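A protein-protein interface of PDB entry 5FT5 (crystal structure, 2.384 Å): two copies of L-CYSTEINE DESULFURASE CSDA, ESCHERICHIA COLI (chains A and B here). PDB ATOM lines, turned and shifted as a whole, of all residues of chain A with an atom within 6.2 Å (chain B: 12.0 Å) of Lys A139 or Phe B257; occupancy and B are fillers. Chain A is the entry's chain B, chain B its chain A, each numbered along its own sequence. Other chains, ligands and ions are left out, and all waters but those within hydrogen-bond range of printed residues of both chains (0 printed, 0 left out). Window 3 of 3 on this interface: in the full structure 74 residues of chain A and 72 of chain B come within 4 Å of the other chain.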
ATOM      1  N   ILE A 112      22.679 -26.825   2.053  1.00  0.00           N
ATOM      2  CA  ILE A 112      22.134 -26.049   0.950  1.00  0.00           C
ATOM      3  C   ILE A 112      23.183 -25.034   0.524  1.00  0.00           C
ATOM      4  O   ILE A 112      23.521 -24.127   1.287  1.00  0.00           O
ATOM      5  CB  ILE A 112      20.848 -25.307   1.373  1.00  0.00           C
ATOM      6  CG1 ILE A 112      19.850 -26.282   2.004  1.00  0.00           C
ATOM      7  CG2 ILE A 112      20.220 -24.595   0.185  1.00  0.00           C
ATOM      8  CD1 ILE A 112      18.786 -25.608   2.836  1.00  0.00           C
ATOM      9  N   ILE A 113      23.707 -25.196  -0.689  1.00  0.00           N
ATOM     10  CA  ILE A 113      24.746 -24.303  -1.189  1.00  0.00           C
ATOM     11  C   ILE A 113      24.121 -23.115  -1.897  1.00  0.00           C
ATOM     12  O   ILE A 113      23.435 -23.275  -2.903  1.00  0.00           O
ATOM     13  CB  ILE A 113      25.718 -25.022  -2.154  1.00  0.00           C
ATOM     14  CG1 ILE A 113      26.277 -26.292  -1.510  1.00  0.00           C
ATOM     15  CG2 ILE A 113      26.857 -24.096  -2.549  1.00  0.00           C
ATOM     16  CD1 ILE A 113      27.190 -27.088  -2.422  1.00  0.00           C
ATOM     17  N   VAL A 114      24.354 -21.924  -1.358  1.00  0.00           N
ATOM     18  CA  VAL A 114      23.848 -20.700  -1.961  1.00  0.00           C
ATOM     19  C   VAL A 114      25.015 -19.812  -2.376  1.00  0.00           C
ATOM     20  O   VAL A 114      25.994 -19.681  -1.639  1.00  0.00           O
ATOM     21  CB  VAL A 114      22.928 -19.930  -0.999  1.00  0.00           C
ATOM     22  CG1 VAL A 114      22.389 -18.668  -1.668  1.00  0.00           C
ATOM     23  CG2 VAL A 114      21.783 -20.825  -0.532  1.00  0.00           C
ATOM     24  N   SER A 115      24.911 -19.218  -3.562  1.00  0.00           N
ATOM     25  CA  SER A 115      25.978 -18.387  -4.103  1.00  0.00           C
ATOM     26  C   SER A 115      25.972 -17.016  -3.451  1.00  0.00           C
ATOM     27  O   SER A 115      24.909 -16.467  -3.153  1.00  0.00           O
ATOM     28  CB  SER A 115      25.834 -18.246  -5.617  1.00  0.00           C
ATOM     29  OG  SER A 115      25.702 -16.885  -5.989  1.00  0.00           O
ATOM     30  N   VAL A 116      27.164 -16.463  -3.243  1.00  0.00           N
ATOM     31  CA  VAL A 116      27.307 -15.178  -2.566  1.00  0.00           C
ATOM     32  C   VAL A 116      26.760 -14.018  -3.394  1.00  0.00           C
ATOM     33  O   VAL A 116      26.545 -12.929  -2.865  1.00  0.00           O
ATOM     34  CB  VAL A 116      28.781 -14.885  -2.206  1.00  0.00           C
ATOM     35  CG1 VAL A 116      29.560 -14.454  -3.444  1.00  0.00           C
ATOM     36  CG2 VAL A 116      28.864 -13.816  -1.126  1.00  0.00           C
ATOM     37  N   ALA A 117      26.531 -14.252  -4.683  1.00  0.00           N
ATOM     38  CA  ALA A 117      26.046 -13.199  -5.577  1.00  0.00           C
ATOM     39  C   ALA A 117      24.527 -13.195  -5.723  1.00  0.00           C
ATOM     40  O   ALA A 117      23.986 -12.534  -6.614  1.00  0.00           O
ATOM     41  CB  ALA A 117      26.695 -13.329  -6.949  1.00  0.00           C
ATOM     42  N   LEU A 123      18.096 -16.370  -1.286  1.00  0.00           N
ATOM     43  CA  LEU A 123      18.949 -16.641  -0.130  1.00  0.00           C
ATOM     44  C   LEU A 123      18.121 -16.774   1.142  1.00  0.00           C
ATOM     45  O   LEU A 123      18.240 -17.760   1.865  1.00  0.00           O
ATOM     46  CB  LEU A 123      20.000 -15.543   0.064  1.00  0.00           C
ATOM     47  CG  LEU A 123      20.743 -15.594   1.410  1.00  0.00           C
ATOM     48  CD1 LEU A 123      21.503 -16.903   1.575  1.00  0.00           C
ATOM     49  CD2 LEU A 123      21.688 -14.407   1.587  1.00  0.00           C
ATOM     50  N   LEU A 127      17.718 -19.768   4.149  1.00  0.00           N
ATOM     51  CA  LEU A 127      18.038 -19.526   5.554  1.00  0.00           C
ATOM     52  C   LEU A 127      16.848 -19.931   6.427  1.00  0.00           C
ATOM     53  O   LEU A 127      17.017 -20.537   7.486  1.00  0.00           O
ATOM     54  CB  LEU A 127      18.406 -18.058   5.780  1.00  0.00           C
ATOM     55  CG  LEU A 127      19.729 -17.601   5.154  1.00  0.00           C
ATOM     56  CD1 LEU A 127      19.823 -16.079   5.100  1.00  0.00           C
ATOM     57  CD2 LEU A 127      20.920 -18.191   5.918  1.00  0.00           C
ATOM     58  N   LYS A 136      21.699 -26.708   6.869  1.00  0.00           N
ATOM     59  CA  LYS A 136      22.359 -25.404   6.834  1.00  0.00           C
ATOM     60  C   LYS A 136      22.839 -24.915   5.470  1.00  0.00           C
ATOM     61  O   LYS A 136      23.046 -25.692   4.540  1.00  0.00           O
ATOM     62  CB  LYS A 136      23.481 -25.296   7.869  1.00  0.00           C
ATOM     63  CG  LYS A 136      23.786 -23.838   8.216  1.00  0.00           C
ATOM     64  CD  LYS A 136      22.574 -22.939   7.882  1.00  0.00           C
ATOM     65  CE  LYS A 136      22.761 -21.495   8.346  1.00  0.00           C
ATOM     66  NZ  LYS A 136      24.072 -20.923   7.921  1.00  0.00           N
ATOM     67  N   VAL A 137      23.012 -23.603   5.383  1.00  0.00           N
ATOM     68  CA  VAL A 137      23.398 -22.934   4.157  1.00  0.00           C
ATOM     69  C   VAL A 137      24.911 -22.844   4.071  1.00  0.00           C
ATOM     70  O   VAL A 137      25.564 -22.311   4.974  1.00  0.00           O
ATOM     71  CB  VAL A 137      22.820 -21.512   4.125  1.00  0.00           C
ATOM     72  CG1 VAL A 137      23.175 -20.817   2.819  1.00  0.00           C
ATOM     73  CG2 VAL A 137      21.319 -21.554   4.331  1.00  0.00           C
ATOM     74  N   VAL A 138      25.470 -23.374   2.990  1.00  0.00           N
ATOM     75  CA  VAL A 138      26.898 -23.268   2.749  1.00  0.00           C
ATOM     76  C   VAL A 138      27.145 -22.234   1.655  1.00  0.00           C
ATOM     77  O   VAL A 138      26.449 -22.215   0.627  1.00  0.00           O
ATOM     78  CB  VAL A 138      27.500 -24.623   2.332  1.00  0.00           C
ATOM     79  CG1 VAL A 138      28.965 -24.456   1.964  1.00  0.00           C
ATOM     80  CG2 VAL A 138      27.336 -25.642   3.440  1.00  0.00           C
ATOM     81  N   LYS A 139      28.134 -21.375   1.868  1.00  0.00           N
ATOM     82  CA  LYS A 139      28.395 -20.283   0.936  1.00  0.00           C
ATOM     83  C   LYS A 139      29.244 -20.691  -0.278  1.00  0.00           C
ATOM     84  O   LYS A 139      30.258 -21.392  -0.151  1.00  0.00           O
ATOM     85  CB  LYS A 139      29.013 -19.074   1.671  1.00  0.00           C
ATOM     86  CG  LYS A 139      28.953 -17.762   0.868  1.00  0.00           C
ATOM     87  CD  LYS A 139      29.388 -16.528   1.701  1.00  0.00           C
ATOM     88  CE  LYS A 139      30.887 -16.488   1.921  1.00  0.00           C
ATOM     89  NZ  LYS A 139      31.346 -15.356   2.772  1.00  0.00           N
ATOM     90  N   LEU A 140      28.786 -20.280  -1.458  1.00  0.00           N
ATOM     91  CA  LEU A 140      29.569 -20.409  -2.672  1.00  0.00           C
ATOM     92  C   LEU A 140      30.082 -19.015  -3.022  1.00  0.00           C
ATOM     93  O   LEU A 140      29.299 -18.135  -3.377  1.00  0.00           O
ATOM     94  CB  LEU A 140      28.723 -20.996  -3.802  1.00  0.00           C
ATOM     95  CG  LEU A 140      29.369 -21.003  -5.186  1.00  0.00           C
ATOM     96  CD1 LEU A 140      30.624 -21.868  -5.197  1.00  0.00           C
ATOM     97  CD2 LEU A 140      28.366 -21.474  -6.234  1.00  0.00           C
ATOM     98  N   PRO A 141      31.403 -18.805  -2.904  1.00  0.00           N
ATOM     99  CA  PRO A 141      32.013 -17.483  -3.077  1.00  0.00           C
ATOM    100  C   PRO A 141      32.290 -17.129  -4.532  1.00  0.00           C
ATOM    101  O   PRO A 141      32.167 -17.966  -5.427  1.00  0.00           O
ATOM    102  CB  PRO A 141      33.339 -17.624  -2.331  1.00  0.00           C
ATOM    103  CG  PRO A 141      33.703 -19.053  -2.531  1.00  0.00           C
ATOM    104  CD  PRO A 141      32.395 -19.817  -2.501  1.00  0.00           C
ATOM    105  N   LEU A 156      33.183 -27.928  -2.256  1.00  0.00           N
ATOM    106  CA  LEU A 156      32.102 -27.524  -1.364  1.00  0.00           C
ATOM    107  C   LEU A 156      31.010 -28.586  -1.205  1.00  0.00           C
ATOM    108  O   LEU A 156      30.198 -28.519  -0.281  1.00  0.00           O
ATOM    109  CB  LEU A 156      31.482 -26.207  -1.836  1.00  0.00           C
ATOM    110  CG  LEU A 156      32.311 -24.939  -1.629  1.00  0.00           C
ATOM    111  CD1 LEU A 156      31.504 -23.717  -2.038  1.00  0.00           C
ATOM    112  CD2 LEU A 156      32.762 -24.823  -0.183  1.00  0.00           C
ATOM    113  N   PRO A 361      25.024  -9.402   0.770  1.00  0.00           N
ATOM    114  CA  PRO A 361      26.188 -10.299   0.782  1.00  0.00           C
ATOM    115  C   PRO A 361      27.118 -10.072  -0.415  1.00  0.00           C
ATOM    116  O   PRO A 361      28.343 -10.066  -0.250  1.00  0.00           O
ATOM    117  CB  PRO A 361      25.564 -11.695   0.702  1.00  0.00           C
ATOM    118  CG  PRO A 361      24.151 -11.512   1.165  1.00  0.00           C
ATOM    119  CD  PRO A 361      23.752 -10.141   0.726  1.00  0.00           C
ATOM    120  N   GLU A 365      31.137  -8.502  -0.356  1.00  0.00           N
ATOM    121  CA  GLU A 365      32.282  -9.113  -1.021  1.00  0.00           C
ATOM    122  C   GLU A 365      33.031  -8.098  -1.873  1.00  0.00           C
ATOM    123  O   GLU A 365      34.256  -8.050  -1.856  1.00  0.00           O
ATOM    124  CB  GLU A 365      31.829 -10.283  -1.897  1.00  0.00           C
ATOM    125  CG  GLU A 365      31.401 -11.513  -1.121  1.00  0.00           C
ATOM    126  CD  GLU A 365      32.573 -12.231  -0.487  1.00  0.00           C
ATOM    127  OE1 GLU A 365      33.684 -12.154  -1.057  1.00  0.00           O
ATOM    128  OE2 GLU A 365      32.383 -12.862   0.580  1.00  0.00           O
ATOM    129  N   VAL B 252      13.037  -8.255   4.657  1.00  0.00           N
ATOM    130  CA  VAL B 252      14.260  -8.325   5.453  1.00  0.00           C
ATOM    131  C   VAL B 252      14.817  -6.952   5.811  1.00  0.00           C
ATOM    132  O   VAL B 252      14.593  -5.965   5.110  1.00  0.00           O
ATOM    133  CB  VAL B 252      15.373  -9.111   4.732  1.00  0.00           C
ATOM    134  CG1 VAL B 252      15.004 -10.579   4.614  1.00  0.00           C
ATOM    135  CG2 VAL B 252      15.654  -8.501   3.364  1.00  0.00           C
ATOM    136  N   HIS B 253      15.552  -6.899   6.912  1.00  0.00           N
ATOM    137  CA  HIS B 253      16.268  -5.694   7.290  1.00  0.00           C
ATOM    138  C   HIS B 253      17.764  -5.907   7.063  1.00  0.00           C
ATOM    139  O   HIS B 253      18.417  -5.134   6.366  1.00  0.00           O
ATOM    140  CB  HIS B 253      15.987  -5.349   8.752  1.00  0.00           C
ATOM    141  CG  HIS B 253      16.670  -4.107   9.223  1.00  0.00           C
ATOM    142  ND1 HIS B 253      17.692  -3.504   8.514  1.00  0.00           N
ATOM    143  CD2 HIS B 253      16.486  -3.348  10.327  1.00  0.00           C
ATOM    144  CE1 HIS B 253      18.104  -2.434   9.163  1.00  0.00           C
ATOM    145  NE2 HIS B 253      17.389  -2.314  10.270  1.00  0.00           N
ATOM    146  N   GLU B 254      18.293  -6.976   7.649  1.00  0.00           N
ATOM    147  CA  GLU B 254      19.701  -7.314   7.512  1.00  0.00           C
ATOM    148  C   GLU B 254      19.840  -8.777   7.109  1.00  0.00           C
ATOM    149  O   GLU B 254      19.207  -9.650   7.698  1.00  0.00           O
ATOM    150  CB  GLU B 254      20.424  -7.068   8.833  1.00  0.00           C
ATOM    151  CG  GLU B 254      21.753  -6.377   8.674  1.00  0.00           C
ATOM    152  CD  GLU B 254      21.619  -5.038   7.983  1.00  0.00           C
ATOM    153  OE1 GLU B 254      21.323  -4.039   8.675  1.00  0.00           O
ATOM    154  OE2 GLU B 254      21.805  -4.988   6.747  1.00  0.00           O
ATOM    155  N   VAL B 255      20.667  -9.046   6.106  1.00  0.00           N
ATOM    156  CA  VAL B 255      20.852 -10.411   5.627  1.00  0.00           C
ATOM    157  C   VAL B 255      22.330 -10.769   5.543  1.00  0.00           C
ATOM    158  O   VAL B 255      23.153  -9.947   5.151  1.00  0.00           O
ATOM    159  CB  VAL B 255      20.239 -10.610   4.222  1.00  0.00           C
ATOM    160  CG1 VAL B 255      20.223 -12.087   3.858  1.00  0.00           C
ATOM    161  CG2 VAL B 255      18.840 -10.018   4.153  1.00  0.00           C
ATOM    162  N   SER B 256      22.659 -12.001   5.914  1.00  0.00           N
ATOM    163  CA  SER B 256      24.004 -12.532   5.723  1.00  0.00           C
ATOM    164  C   SER B 256      23.917 -14.049   5.710  1.00  0.00           C
ATOM    165  O   SER B 256      22.834 -14.609   5.835  1.00  0.00           O
ATOM    166  CB  SER B 256      24.947 -12.069   6.834  1.00  0.00           C
ATOM    167  OG  SER B 256      24.784 -12.863   7.999  1.00  0.00           O
ATOM    168  N   PHE B 257      25.051 -14.723   5.569  1.00  0.00           N
ATOM    169  CA  PHE B 257      25.037 -16.180   5.549  1.00  0.00           C
ATOM    170  C   PHE B 257      24.895 -16.813   6.935  1.00  0.00           C
ATOM    171  O   PHE B 257      24.859 -18.035   7.063  1.00  0.00           O
ATOM    172  CB  PHE B 257      26.241 -16.725   4.779  1.00  0.00           C
ATOM    173  CG  PHE B 257      26.030 -16.747   3.296  1.00  0.00           C
ATOM    174  CD1 PHE B 257      25.941 -15.564   2.582  1.00  0.00           C
ATOM    175  CD2 PHE B 257      25.884 -17.946   2.620  1.00  0.00           C
ATOM    176  CE1 PHE B 257      25.729 -15.577   1.219  1.00  0.00           C
ATOM    177  CE2 PHE B 257      25.671 -17.964   1.251  1.00  0.00           C
ATOM    178  CZ  PHE B 257      25.592 -16.778   0.553  1.00  0.00           C
ATOM    179  N   ASP B 258      24.784 -15.975   7.964  1.00  0.00           N
ATOM    180  CA  ASP B 258      24.584 -16.449   9.333  1.00  0.00           C
ATOM    181  C   ASP B 258      23.115 -16.382   9.731  1.00  0.00           C
ATOM    182  O   ASP B 258      22.698 -16.984  10.723  1.00  0.00           O
ATOM    183  CB  ASP B 258      25.402 -15.616  10.317  1.00  0.00           C
ATOM    184  CG  ASP B 258      26.884 -15.701  10.058  1.00  0.00           C
ATOM    185  OD1 ASP B 258      27.364 -16.797   9.698  1.00  0.00           O
ATOM    186  OD2 ASP B 258      27.569 -14.667  10.216  1.00  0.00           O
ATOM    187  N   GLY B 259      22.333 -15.637   8.960  1.00  0.00           N
ATOM    188  CA  GLY B 259      20.925 -15.461   9.251  1.00  0.00           C
ATOM    189  C   GLY B 259      20.483 -14.060   8.889  1.00  0.00           C
ATOM    190  O   GLY B 259      21.215 -13.328   8.220  1.00  0.00           O
ATOM    191  N   PHE B 260      19.293 -13.678   9.341  1.00  0.00           N
ATOM    192  CA  PHE B 260      18.712 -12.400   8.951  1.00  0.00           C
ATOM    193  C   PHE B 260      17.804 -11.814  10.023  1.00  0.00           C
ATOM    194  O   PHE B 260      17.414 -12.499  10.970  1.00  0.00           O
ATOM    195  CB  PHE B 260      17.916 -12.568   7.656  1.00  0.00           C
ATOM    196  CG  PHE B 260      16.712 -13.461   7.797  1.00  0.00           C
ATOM    197  CD1 PHE B 260      16.831 -14.836   7.668  1.00  0.00           C
ATOM    198  CD2 PHE B 260      15.459 -12.922   8.063  1.00  0.00           C
ATOM    199  CE1 PHE B 260      15.726 -15.659   7.798  1.00  0.00           C
ATOM    200  CE2 PHE B 260      14.347 -13.740   8.195  1.00  0.00           C
ATOM    201  CZ  PHE B 260      14.481 -15.110   8.063  1.00  0.00           C
ATOM    202  N   THR B 261      17.476 -10.535   9.861  1.00  0.00           N
ATOM    203  CA  THR B 261      16.465  -9.876  10.681  1.00  0.00           C
ATOM    204  C   THR B 261      15.376  -9.321   9.767  1.00  0.00           C
ATOM    205  O   THR B 261      15.642  -9.000   8.609  1.00  0.00           O
ATOM    206  CB  THR B 261      17.070  -8.733  11.503  1.00  0.00           C
ATOM    207  OG1 THR B 261      17.773  -7.839  10.630  1.00  0.00           O
ATOM    208  CG2 THR B 261      18.039  -9.285  12.537  1.00  0.00           C
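The side-chain amino group (NZ) of Lys A136 sits at hydrogen-bond distance from the backbone carbonyl oxygen (O) of Phe B257 (3.1 Å).
N of Ile A112 lies within hydrogen-bond range of O of Lys A136 (2.8 Å). The backbone NH (N) of Val A114 is in hydrogen-bond range of the backbone carbonyl oxygen (O) of Val A138, 2.9 Å away. The backbone carbonyl oxygen of Val A114 lies within hydrogen-bond range of the backbone NH of Leu A140, 2.9 Å away. The side-chain hydroxyl (OG) of Ser A115 lies within hydrogen-bond range of the backbone NH (N) of Ala A117 (3.1 Å). N of Val A116 is in hydrogen-bond range of O of Leu A140 (2.7 Å). The side-chain amino group (NZ) of Lys A139 lies within salt-bridge range of the side-chain carboxylate (OE2) of Glu A365 (3.5 Å).
Phe B257 touches Val A114. Phe B257 touches Ser A115. Phe B257 touches Val A116 (CZ to CA, 3.9 Å). Val B255 touches Leu A123. Leu A127 touches Ser B256 (CD1 to O, 3.4 Å). Val A137 touches Phe B257. Lys A139 touches Phe B257 (CG to CE2, 3.3 Å). CE1 of Phe B257 touches CB of Pro A361, 3.9 Å away.
Of chain B, only Phe B257 (3.4 Å) comes within 4 Å of Val A114. Ser A115 touches just one residue of chain B: Phe B257. Leu A123 touches just one residue of chain B: Val B255. Printed residues of chain B within 4 Å of Leu A127: Ser B256. Printed residues of chain B within 4 Å of Lys A136: Phe B257 (3.1 Å). No residue of chain B comes within 4 Å of Val A138. No residue of chain B comes within 4 Å of Pro A141. No residue of chain B comes within 4 Å of Leu A156. Of the printed residues of chain B, Pro A361 touches Phe B257 (3.9 Å). Printed residues of chain A within 4 Å of Val B255: Leu A123. Of the printed residues of chain A, Ser B256 touches Leu A127 (3.4 Å). Printed residues of chain A within 4 Å of Phe B257: Val A114, Ser A115, Val A116, Lys A136, Val A137, Lys A139 and Pro A361. Phe B260 touches none of the printed residues of chain A. The nearest residue of chain A that does not touch Phe B257 is Leu A127 (4.1 Å).
Hydrophobic or aromatic side chains of chain B that line the printed part of chain A: Val B255 and Phe B257. Of the 17 printed residues of chain A, 9 touch a printed residue of chain B. Printed residues of chain A that touch a printed residue of chain B: Val A114, Ser A115, Val A116, Leu A123, Leu A127, Lys A136, Val A137, Lys A139 and Pro A361. Hydrophobic or aromatic side chains of chain A that line the printed part of chain B: Leu A123, Leu A127, Val A137 and Pro A361. Among the printed residues, 9 pairs touch across the chains.
No position is printed for both chains. Of the 9 pairs that touch across the chains among the printed residues, none has its exchanged pair printed and touching as well.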
